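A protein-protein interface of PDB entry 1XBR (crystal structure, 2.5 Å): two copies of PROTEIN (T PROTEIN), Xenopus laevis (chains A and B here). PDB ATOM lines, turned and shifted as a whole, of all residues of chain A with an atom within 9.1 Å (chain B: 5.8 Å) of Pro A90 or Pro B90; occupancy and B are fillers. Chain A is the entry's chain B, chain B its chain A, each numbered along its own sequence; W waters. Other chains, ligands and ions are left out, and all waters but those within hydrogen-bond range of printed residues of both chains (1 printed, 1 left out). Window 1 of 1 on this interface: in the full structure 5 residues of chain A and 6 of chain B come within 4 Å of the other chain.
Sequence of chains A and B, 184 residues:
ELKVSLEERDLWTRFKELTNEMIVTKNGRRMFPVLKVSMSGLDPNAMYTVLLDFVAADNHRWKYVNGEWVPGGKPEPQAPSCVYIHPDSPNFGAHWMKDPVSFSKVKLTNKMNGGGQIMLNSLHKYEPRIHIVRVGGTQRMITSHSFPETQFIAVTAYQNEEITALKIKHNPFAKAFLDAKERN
Of the 10 printed residues of chain B, 6 touch a printed residue of chain A.
Hydrophobic or aromatic side chains of chain B within 4 Å of the printed part of chain A: Met B47, Pro B90, Phe B92 and Val B135.
Among the printed residues, 11 pairs touch across the chains.
Among the printed residues, no Asp or Glu carboxylate lies within 4 Å of a Lys or Arg side-chain nitrogen of the other chain.
Pro A90 touches just these residues of chain B: Met B47 (3.7 Å), Pro B90 (3.2 Å), Asn B91 (3.3 Å) and Phe B92 (3.9 Å).
Of the printed residues of chain A, Ser B89 touches Asn A91.
Asn B91 touches just these residues of chain A: Ser A89 (3.5 Å) and Pro A90 (3.3 Å).
Of the printed residues of chain A, Phe B92 touches Pro A90 (3.9 Å).
Printed residues of chain A within 4 Å of Met B47: Met A47 and Pro A90.
Thr A49 touches none of the printed residues of chain B.
The nearest residue of chain B that does not touch Pro A90 is Ser B89 (5.0 Å).
The backbone NH (N) of Asn B91 lies close to the side-chain sulfur (SD) of Met B47, 3.6 Å away.
ND2 of Asn B91 sits close to O of Asp B88, 3.2 Å away.
The indole nitrogen (NE1) of Trp B96 is in hydrogen-bond range of the backbone carbonyl oxygen (O) of Asn B91 (2.8 Å).
The backbone NH (N) of Asn A91 is in hydrogen-bond range of the side-chain sulfur (SD) of Met A47, 3.5 Å away.
O of Met A47 sits at hydrogen-bond distance from N of Val A135 (2.9 Å).
OG of Ser A89 is in hydrogen-bond range of O of His A86 (3.2 Å).
O of Ser B89 is in hydrogen-bond range of ND2 of Asn A91.
The side-chain amide nitrogen (ND2) of Asn B91 sits at hydrogen-bond distance from the backbone carbonyl oxygen (O) of Ser A89, 3.5 Å away.
The backbone carbonyl oxygen (O) of Pro A90 lies close to the backbone carbonyl oxygen (O) of Pro B90 (3.2 Å).
Among the printed residues, merely in contact across the chains: Met A47 with Met B47 (3.3 Å), Met A47 with Pro B90 (3.7 Å), Pro A90 with Met B47 (3.7 Å), Pro A90 with Asn B91 (3.3 Å), Pro A90 with Phe B92 (3.9 Å), Asn A91 with Pro B90 (3.5 Å), Phe A92 with Pro B90 (3.8 Å) and Phe A92 with Val B135 (3.9 Å).
Met B47 touches its own counterpart, Met A47.
Met A47 touches Pro B90, and with the chains exchanged Pro A90 touches Met B47.
Ser A89 touches Asn B91, and with the chains exchanged Asn A91 touches Ser B89.
Pro A90 touches Asn B91, and with the chains exchanged Asn A91 touches Pro B90.
Of the 11 pairs that touch across the chains among the printed residues, 10 have their exchanged pair printed and touching as well.
Water W1 lies within hydrogen-bond range of the backbone carbonyl oxygen (O) of Pro A87 (2.7 Å), the side-chain amide nitrogen (ND2) of Asn B91 (3.3 Å) and the backbone carbonyl oxygen (O) of Ser A89 (3.4 Å).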
ATOM      1  N   ASN A  45      11.416  18.138 -15.049  1.00  0.00           N
ATOM      2  CA  ASN A  45      11.487  19.541 -15.447  1.00  0.00           C
ATOM      3  C   ASN A  45      12.882  20.117 -15.551  1.00  0.00           C
ATOM      4  O   ASN A  45      13.059  21.234 -16.060  1.00  0.00           O
ATOM      5  CB  ASN A  45      10.669  20.394 -14.487  1.00  0.00           C
ATOM      6  CG  ASN A  45       9.274  19.847 -14.262  1.00  0.00           C
ATOM      7  OD1 ASN A  45       8.337  20.174 -14.991  1.00  0.00           O
ATOM      8  ND2 ASN A  45       9.131  19.008 -13.246  1.00  0.00           N
ATOM      9  N   ALA A  46      13.868  19.381 -15.050  1.00  0.00           N
ATOM     10  CA  ALA A  46      15.254  19.830 -15.104  1.00  0.00           C
ATOM     11  C   ALA A  46      15.835  19.604 -16.508  1.00  0.00           C
ATOM     12  O   ALA A  46      15.380  18.715 -17.248  1.00  0.00           O
ATOM     13  CB  ALA A  46      16.072  19.090 -14.082  1.00  0.00           C
ATOM     14  N   MET A  47      16.843  20.401 -16.856  1.00  0.00           N
ATOM     15  CA  MET A  47      17.517  20.321 -18.149  1.00  0.00           C
ATOM     16  C   MET A  47      18.749  19.418 -18.014  1.00  0.00           C
ATOM     17  O   MET A  47      19.532  19.582 -17.072  1.00  0.00           O
ATOM     18  CB  MET A  47      17.960  21.721 -18.596  1.00  0.00           C
ATOM     19  CG  MET A  47      18.341  21.856 -20.080  1.00  0.00           C
ATOM     20  SD  MET A  47      16.927  21.710 -21.188  1.00  0.00           S
ATOM     21  CE  MET A  47      16.221  23.365 -21.057  1.00  0.00           C
ATOM     22  N   TYR A  48      18.914  18.476 -18.946  1.00  0.00           N
ATOM     23  CA  TYR A  48      20.045  17.547 -18.939  1.00  0.00           C
ATOM     24  C   TYR A  48      20.694  17.413 -20.315  1.00  0.00           C
ATOM     25  O   TYR A  48      20.040  17.581 -21.358  1.00  0.00           O
ATOM     26  CB  TYR A  48      19.603  16.146 -18.512  1.00  0.00           C
ATOM     27  CG  TYR A  48      18.918  16.061 -17.167  1.00  0.00           C
ATOM     28  CD1 TYR A  48      19.653  15.837 -16.003  1.00  0.00           C
ATOM     29  CD2 TYR A  48      17.531  16.152 -17.058  1.00  0.00           C
ATOM     30  CE1 TYR A  48      19.021  15.696 -14.758  1.00  0.00           C
ATOM     31  CE2 TYR A  48      16.884  16.015 -15.816  1.00  0.00           C
ATOM     32  CZ  TYR A  48      17.641  15.786 -14.670  1.00  0.00           C
ATOM     33  OH  TYR A  48      17.026  15.640 -13.444  1.00  0.00           O
ATOM     34  N   THR A  49      21.986  17.100 -20.292  1.00  0.00           N
ATOM     35  CA  THR A  49      22.779  16.862 -21.486  1.00  0.00           C
ATOM     36  C   THR A  49      23.338  15.455 -21.289  1.00  0.00           C
ATOM     37  O   THR A  49      23.802  15.120 -20.200  1.00  0.00           O
ATOM     38  CB  THR A  49      23.914  17.869 -21.632  1.00  0.00           C
ATOM     39  OG1 THR A  49      23.379  19.111 -22.096  1.00  0.00           O
ATOM     40  CG2 THR A  49      24.935  17.382 -22.626  1.00  0.00           C
ATOM     41  N   VAL A  50      23.191  14.615 -22.310  1.00  0.00           N
ATOM     42  CA  VAL A  50      23.663  13.245 -22.261  1.00  0.00           C
ATOM     43  C   VAL A  50      24.926  13.126 -23.104  1.00  0.00           C
ATOM     44  O   VAL A  50      24.978  13.620 -24.223  1.00  0.00           O
ATOM     45  CB  VAL A  50      22.573  12.304 -22.749  1.00  0.00           C
ATOM     46  CG1 VAL A  50      23.064  10.871 -22.775  1.00  0.00           C
ATOM     47  CG2 VAL A  50      21.371  12.432 -21.833  1.00  0.00           C
ATOM     48  N   ILE A  85      28.330  14.226 -27.824  1.00  0.00           N
ATOM     49  CA  ILE A  85      27.146  14.829 -27.221  1.00  0.00           C
ATOM     50  C   ILE A  85      25.891  14.285 -27.878  1.00  0.00           C
ATOM     51  O   ILE A  85      25.665  14.540 -29.059  1.00  0.00           O
ATOM     52  CB  ILE A  85      27.115  16.370 -27.433  1.00  0.00           C
ATOM     53  CG1 ILE A  85      28.417  17.008 -26.959  1.00  0.00           C
ATOM     54  CG2 ILE A  85      25.966  16.984 -26.659  1.00  0.00           C
ATOM     55  CD1 ILE A  85      28.457  18.497 -27.161  1.00  0.00           C
ATOM     56  N   HIS A  86      25.054  13.571 -27.131  1.00  0.00           N
ATOM     57  CA  HIS A  86      23.829  13.057 -27.717  1.00  0.00           C
ATOM     58  C   HIS A  86      23.099  14.217 -28.412  1.00  0.00           C
ATOM     59  O   HIS A  86      22.792  15.228 -27.797  1.00  0.00           O
ATOM     60  CB  HIS A  86      22.937  12.416 -26.665  1.00  0.00           C
ATOM     61  CG  HIS A  86      21.790  11.651 -27.249  1.00  0.00           C
ATOM     62  ND1 HIS A  86      20.706  12.269 -27.838  1.00  0.00           N
ATOM     63  CD2 HIS A  86      21.565  10.320 -27.352  1.00  0.00           C
ATOM     64  CE1 HIS A  86      19.863  11.353 -28.278  1.00  0.00           C
ATOM     65  NE2 HIS A  86      20.360  10.161 -27.996  1.00  0.00           N
ATOM     66  N   PRO A  87      22.797  14.065 -29.709  1.00  0.00           N
ATOM     67  CA  PRO A  87      22.116  15.092 -30.494  1.00  0.00           C
ATOM     68  C   PRO A  87      20.863  15.755 -29.904  1.00  0.00           C
ATOM     69  O   PRO A  87      20.519  16.862 -30.306  1.00  0.00           O
ATOM     70  CB  PRO A  87      21.837  14.373 -31.817  1.00  0.00           C
ATOM     71  CG  PRO A  87      21.752  12.935 -31.419  1.00  0.00           C
ATOM     72  CD  PRO A  87      22.936  12.836 -30.507  1.00  0.00           C
ATOM     73  N   ASP A  88      20.187  15.100 -28.963  1.00  0.00           N
ATOM     74  CA  ASP A  88      18.971  15.680 -28.349  1.00  0.00           C
ATOM     75  C   ASP A  88      19.250  16.708 -27.231  1.00  0.00           C
ATOM     76  O   ASP A  88      18.315  17.295 -26.678  1.00  0.00           O
ATOM     77  CB  ASP A  88      18.068  14.594 -27.768  1.00  0.00           C
ATOM     78  CG  ASP A  88      17.390  13.729 -28.827  1.00  0.00           C
ATOM     79  OD1 ASP A  88      17.830  13.680 -30.004  1.00  0.00           O
ATOM     80  OD2 ASP A  88      16.417  13.043 -28.451  1.00  0.00           O
ATOM     81  N   SER A  89      20.521  16.860 -26.859  1.00  0.00           N
ATOM     82  CA  SER A  89      20.962  17.787 -25.815  1.00  0.00           C
ATOM     83  C   SER A  89      21.033  19.240 -26.287  1.00  0.00           C
ATOM     84  O   SER A  89      21.516  19.520 -27.389  1.00  0.00           O
ATOM     85  CB  SER A  89      22.346  17.369 -25.304  1.00  0.00           C
ATOM     86  OG  SER A  89      22.294  16.074 -24.743  1.00  0.00           O
ATOM     87  N   PRO A  90      20.654  20.196 -25.420  1.00  0.00           N
ATOM     88  CA  PRO A  90      20.164  19.983 -24.054  1.00  0.00           C
ATOM     89  C   PRO A  90      18.683  19.697 -24.093  1.00  0.00           C
ATOM     90  O   PRO A  90      18.017  20.087 -25.050  1.00  0.00           O
ATOM     91  CB  PRO A  90      20.467  21.316 -23.379  1.00  0.00           C
ATOM     92  CG  PRO A  90      20.235  22.294 -24.466  1.00  0.00           C
ATOM     93  CD  PRO A  90      20.868  21.634 -25.682  1.00  0.00           C
ATOM     94  N   ASN A  91      18.160  19.009 -23.082  1.00  0.00           N
ATOM     95  CA  ASN A  91      16.747  18.706 -23.092  1.00  0.00           C
ATOM     96  C   ASN A  91      16.184  18.273 -21.724  1.00  0.00           C
ATOM     97  O   ASN A  91      16.913  17.787 -20.857  1.00  0.00           O
ATOM     98  CB  ASN A  91      16.474  17.653 -24.167  1.00  0.00           C
ATOM     99  CG  ASN A  91      15.121  17.820 -24.809  1.00  0.00           C
ATOM    100  OD1 ASN A  91      14.087  17.708 -24.144  1.00  0.00           O
ATOM    101  ND2 ASN A  91      15.113  18.101 -26.106  1.00  0.00           N
ATOM    102  N   PHE A  92      14.873  18.427 -21.559  1.00  0.00           N
ATOM    103  CA  PHE A  92      14.192  18.112 -20.312  1.00  0.00           C
ATOM    104  C   PHE A  92      14.253  16.655 -19.884  1.00  0.00           C
ATOM    105  O   PHE A  92      14.258  15.749 -20.714  1.00  0.00           O
ATOM    106  CB  PHE A  92      12.727  18.557 -20.398  1.00  0.00           C
ATOM    107  CG  PHE A  92      12.552  20.031 -20.666  1.00  0.00           C
ATOM    108  CD1 PHE A  92      12.710  20.965 -19.647  1.00  0.00           C
ATOM    109  CD2 PHE A  92      12.242  20.487 -21.941  1.00  0.00           C
ATOM    110  CE1 PHE A  92      12.562  22.339 -19.897  1.00  0.00           C
ATOM    111  CE2 PHE A  92      12.091  21.856 -22.202  1.00  0.00           C
ATOM    112  CZ  PHE A  92      12.255  22.785 -21.173  1.00  0.00           C
ATOM    113  N   GLY A  93      14.221  16.432 -18.579  1.00  0.00           N
ATOM    114  CA  GLY A  93      14.259  15.084 -18.067  1.00  0.00           C
ATOM    115  C   GLY A  93      13.118  14.261 -18.612  1.00  0.00           C
ATOM    116  O   GLY A  93      13.279  13.078 -18.909  1.00  0.00           O
ATOM    117  N   HIS A  95      11.753  14.411 -21.483  1.00  0.00           N
ATOM    118  CA  HIS A  95      12.098  13.969 -22.822  1.00  0.00           C
ATOM    119  C   HIS A  95      13.012  12.733 -22.782  1.00  0.00           C
ATOM    120  O   HIS A  95      12.803  11.772 -23.529  1.00  0.00           O
ATOM    121  CB  HIS A  95      12.790  15.101 -23.585  1.00  0.00           C
ATOM    122  CG  HIS A  95      13.364  14.676 -24.900  1.00  0.00           C
ATOM    123  ND1 HIS A  95      14.679  14.290 -25.046  1.00  0.00           N
ATOM    124  CD2 HIS A  95      12.800  14.553 -26.127  1.00  0.00           C
ATOM    125  CE1 HIS A  95      14.901  13.946 -26.301  1.00  0.00           C
ATOM    126  NE2 HIS A  95      13.777  14.095 -26.979  1.00  0.00           N
ATOM    127  N   TRP A  96      14.016  12.766 -21.908  1.00  0.00           N
ATOM    128  CA  TRP A  96      14.963  11.669 -21.789  1.00  0.00           C
ATOM    129  C   TRP A  96      14.353  10.367 -21.268  1.00  0.00           C
ATOM    130  O   TRP A  96      14.798   9.272 -21.633  1.00  0.00           O
ATOM    131  CB  TRP A  96      16.143  12.095 -20.918  1.00  0.00           C
ATOM    132  CG  TRP A  96      16.965  13.252 -21.465  1.00  0.00           C
ATOM    133  CD1 TRP A  96      17.121  14.475 -20.893  1.00  0.00           C
ATOM    134  CD2 TRP A  96      17.800  13.247 -22.641  1.00  0.00           C
ATOM    135  NE1 TRP A  96      18.005  15.235 -21.626  1.00  0.00           N
ATOM    136  CE2 TRP A  96      18.435  14.503 -22.705  1.00  0.00           C
ATOM    137  CE3 TRP A  96      18.080  12.296 -23.638  1.00  0.00           C
ATOM    138  CZ2 TRP A  96      19.331  14.845 -23.732  1.00  0.00           C
ATOM    139  CZ3 TRP A  96      18.968  12.633 -24.655  1.00  0.00           C
ATOM    140  CH2 TRP A  96      19.584  13.898 -24.691  1.00  0.00           C
ATOM    141  N   VAL A 133      24.392  14.777 -17.452  1.00  0.00           N
ATOM    142  CA  VAL A 133      24.815  16.011 -16.805  1.00  0.00           C
ATOM    143  C   VAL A 133      23.660  16.982 -16.661  1.00  0.00           C
ATOM    144  O   VAL A 133      23.066  17.371 -17.658  1.00  0.00           O
ATOM    145  CB  VAL A 133      25.912  16.688 -17.641  1.00  0.00           C
ATOM    146  CG1 VAL A 133      26.173  18.088 -17.155  1.00  0.00           C
ATOM    147  CG2 VAL A 133      27.180  15.858 -17.604  1.00  0.00           C
ATOM    148  N   ARG A 134      23.335  17.360 -15.426  1.00  0.00           N
ATOM    149  CA  ARG A 134      22.264  18.323 -15.174  1.00  0.00           C
ATOM    150  C   ARG A 134      22.778  19.730 -15.423  1.00  0.00           C
ATOM    151  O   ARG A 134      23.699  20.192 -14.744  1.00  0.00           O
ATOM    152  CB  ARG A 134      21.742  18.222 -13.744  1.00  0.00           C
ATOM    153  CG  ARG A 134      20.614  19.207 -13.399  1.00  0.00           C
ATOM    154  CD  ARG A 134      19.906  18.706 -12.156  1.00  0.00           C
ATOM    155  NE  ARG A 134      18.810  19.548 -11.673  1.00  0.00           N
ATOM    156  CZ  ARG A 134      17.813  19.084 -10.918  1.00  0.00           C
ATOM    157  NH1 ARG A 134      17.797  17.798 -10.584  1.00  0.00           N
ATOM    158  NH2 ARG A 134      16.834  19.887 -10.497  1.00  0.00           N
ATOM    159  N   VAL A 135      22.192  20.390 -16.418  1.00  0.00           N
ATOM    160  CA  VAL A 135      22.553  21.753 -16.794  1.00  0.00           C
ATOM    161  C   VAL A 135      22.230  22.678 -15.617  1.00  0.00           C
ATOM    162  O   VAL A 135      21.067  22.852 -15.247  1.00  0.00           O
ATOM    163  CB  VAL A 135      21.780  22.204 -18.066  1.00  0.00           C
ATOM    164  CG1 VAL A 135      22.089  23.652 -18.391  1.00  0.00           C
ATOM    165  CG2 VAL A 135      22.139  21.324 -19.244  1.00  0.00           C
ATOM    166  N   GLY A 136      23.274  23.243 -15.020  1.00  0.00           N
ATOM    167  CA  GLY A 136      23.090  24.115 -13.875  1.00  0.00           C
ATOM    168  C   GLY A 136      23.243  23.344 -12.574  1.00  0.00           C
ATOM    169  O   GLY A 136      23.289  23.947 -11.509  1.00  0.00           O
ATOM    170  N   MET B  47      18.332  30.097 -23.179  1.00  0.00           N
ATOM    171  CA  MET B  47      17.711  28.903 -23.746  1.00  0.00           C
ATOM    172  C   MET B  47      16.475  29.312 -24.536  1.00  0.00           C
ATOM    173  O   MET B  47      15.625  30.019 -24.012  1.00  0.00           O
ATOM    174  CB  MET B  47      17.304  27.943 -22.630  1.00  0.00           C
ATOM    175  CG  MET B  47      16.907  26.556 -23.104  1.00  0.00           C
ATOM    176  SD  MET B  47      18.301  25.649 -23.750  1.00  0.00           S
ATOM    177  CE  MET B  47      18.882  24.936 -22.308  1.00  0.00           C
ATOM    178  N   TYR B  48      16.383  28.878 -25.789  1.00  0.00           N
ATOM    179  CA  TYR B  48      15.243  29.188 -26.646  1.00  0.00           C
ATOM    180  C   TYR B  48      14.640  27.956 -27.346  1.00  0.00           C
ATOM    181  O   TYR B  48      15.330  26.966 -27.638  1.00  0.00           O
ATOM    182  CB  TYR B  48      15.644  30.165 -27.741  1.00  0.00           C
ATOM    183  CG  TYR B  48      16.234  31.462 -27.273  1.00  0.00           C
ATOM    184  CD1 TYR B  48      15.421  32.567 -27.028  1.00  0.00           C
ATOM    185  CD2 TYR B  48      17.612  31.619 -27.171  1.00  0.00           C
ATOM    186  CE1 TYR B  48      15.967  33.808 -26.688  1.00  0.00           C
ATOM    187  CE2 TYR B  48      18.169  32.841 -26.833  1.00  0.00           C
ATOM    188  CZ  TYR B  48      17.339  33.939 -26.602  1.00  0.00           C
ATOM    189  OH  TYR B  48      17.894  35.165 -26.309  1.00  0.00           O
ATOM    190  N   THR B  49      13.346  28.048 -27.633  1.00  0.00           N
ATOM    191  CA  THR B  49      12.609  27.019 -28.344  1.00  0.00           C
ATOM    192  C   THR B  49      12.003  27.709 -29.580  1.00  0.00           C
ATOM    193  O   THR B  49      11.419  28.798 -29.459  1.00  0.00           O
ATOM    194  CB  THR B  49      11.501  26.418 -27.466  1.00  0.00           C
ATOM    195  OG1 THR B  49      12.076  25.470 -26.554  1.00  0.00           O
ATOM    196  CG2 THR B  49      10.442  25.726 -28.324  1.00  0.00           C
ATOM    197  N   ASP B  88      15.224  20.842 -32.819  1.00  0.00           N
ATOM    198  CA  ASP B  88      16.460  21.216 -32.098  1.00  0.00           C
ATOM    199  C   ASP B  88      16.154  21.864 -30.733  1.00  0.00           C
ATOM    200  O   ASP B  88      17.074  22.288 -30.024  1.00  0.00           O
ATOM    201  CB  ASP B  88      17.280  22.240 -32.899  1.00  0.00           C
ATOM    202  CG  ASP B  88      18.017  21.645 -34.107  1.00  0.00           C
ATOM    203  OD1 ASP B  88      17.785  20.487 -34.493  1.00  0.00           O
ATOM    204  OD2 ASP B  88      18.825  22.385 -34.706  1.00  0.00           O
ATOM    205  N   SER B  89      14.869  21.995 -30.406  1.00  0.00           N
ATOM    206  CA  SER B  89      14.419  22.624 -29.174  1.00  0.00           C
ATOM    207  C   SER B  89      14.347  21.690 -27.967  1.00  0.00           C
ATOM    208  O   SER B  89      13.940  20.529 -28.099  1.00  0.00           O
ATOM    209  CB  SER B  89      13.036  23.250 -29.403  1.00  0.00           C
ATOM    210  OG  SER B  89      13.067  24.251 -30.411  1.00  0.00           O
ATOM    211  N   PRO B  90      14.688  22.203 -26.759  1.00  0.00           N
ATOM    212  CA  PRO B  90      15.128  23.579 -26.485  1.00  0.00           C
ATOM    213  C   PRO B  90      16.620  23.713 -26.725  1.00  0.00           C
ATOM    214  O   PRO B  90      17.351  22.728 -26.641  1.00  0.00           O
ATOM    215  CB  PRO B  90      14.801  23.744 -25.016  1.00  0.00           C
ATOM    216  CG  PRO B  90      15.071  22.361 -24.481  1.00  0.00           C
ATOM    217  CD  PRO B  90      14.384  21.501 -25.497  1.00  0.00           C
ATOM    218  N   ASN B  91      17.097  24.919 -27.011  1.00  0.00           N
ATOM    219  CA  ASN B  91      18.518  25.041 -27.250  1.00  0.00           C
ATOM    220  C   ASN B  91      19.060  26.451 -27.080  1.00  0.00           C
ATOM    221  O   ASN B  91      18.308  27.407 -27.126  1.00  0.00           O
ATOM    222  CB  ASN B  91      18.859  24.473 -28.621  1.00  0.00           C
ATOM    223  CG  ASN B  91      20.115  23.667 -28.598  1.00  0.00           C
ATOM    224  OD1 ASN B  91      21.196  24.209 -28.422  1.00  0.00           O
ATOM    225  ND2 ASN B  91      19.987  22.364 -28.729  1.00  0.00           N
ATOM    226  N   PHE B  92      20.374  26.568 -26.898  1.00  0.00           N
ATOM    227  CA  PHE B  92      21.025  27.859 -26.681  1.00  0.00           C
ATOM    228  C   PHE B  92      20.948  28.820 -27.854  1.00  0.00           C
ATOM    229  O   PHE B  92      20.969  28.405 -29.018  1.00  0.00           O
ATOM    230  CB  PHE B  92      22.498  27.663 -26.294  1.00  0.00           C
ATOM    231  CG  PHE B  92      22.692  26.833 -25.072  1.00  0.00           C
ATOM    232  CD1 PHE B  92      22.398  27.356 -23.809  1.00  0.00           C
ATOM    233  CD2 PHE B  92      23.127  25.513 -25.173  1.00  0.00           C
ATOM    234  CE1 PHE B  92      22.535  26.572 -22.660  1.00  0.00           C
ATOM    235  CE2 PHE B  92      23.269  24.717 -24.037  1.00  0.00           C
ATOM    236  CZ  PHE B  92      22.970  25.246 -22.772  1.00  0.00           C
ATOM    237  N   TRP B  96      21.264  28.317 -32.100  1.00  0.00           N
ATOM    238  CA  TRP B  96      20.291  28.858 -33.042  1.00  0.00           C
ATOM    239  C   TRP B  96      20.880  29.843 -34.062  1.00  0.00           C
ATOM    240  O   TRP B  96      20.329  30.009 -35.159  1.00  0.00           O
ATOM    241  CB  TRP B  96      19.163  29.547 -32.265  1.00  0.00           C
ATOM    242  CG  TRP B  96      18.317  28.619 -31.467  1.00  0.00           C
ATOM    243  CD1 TRP B  96      18.153  28.626 -30.114  1.00  0.00           C
ATOM    244  CD2 TRP B  96      17.495  27.550 -31.971  1.00  0.00           C
ATOM    245  NE1 TRP B  96      17.274  27.629 -29.739  1.00  0.00           N
ATOM    246  CE2 TRP B  96      16.856  26.955 -30.862  1.00  0.00           C
ATOM    247  CE3 TRP B  96      17.227  27.043 -33.257  1.00  0.00           C
ATOM    248  CZ2 TRP B  96      15.971  25.875 -30.995  1.00  0.00           C
ATOM    249  CZ3 TRP B  96      16.343  25.968 -33.388  1.00  0.00           C
ATOM    250  CH2 TRP B  96      15.727  25.402 -32.262  1.00  0.00           C
ATOM    251  N   VAL B 135      13.135  30.193 -23.004  1.00  0.00           N
ATOM    252  CA  VAL B 135      12.887  29.072 -22.094  1.00  0.00           C
ATOM    253  C   VAL B 135      13.552  29.345 -20.737  1.00  0.00           C
ATOM    254  O   VAL B 135      14.692  29.813 -20.679  1.00  0.00           O
ATOM    255  CB  VAL B 135      13.438  27.730 -22.691  1.00  0.00           C
ATOM    256  CG1 VAL B 135      13.163  26.565 -21.752  1.00  0.00           C
ATOM    257  CG2 VAL B 135      12.810  27.455 -24.037  1.00  0.00           C
HETATM  258  O   HOH W   1      19.589  19.430 -30.209  1.00  0.00           O
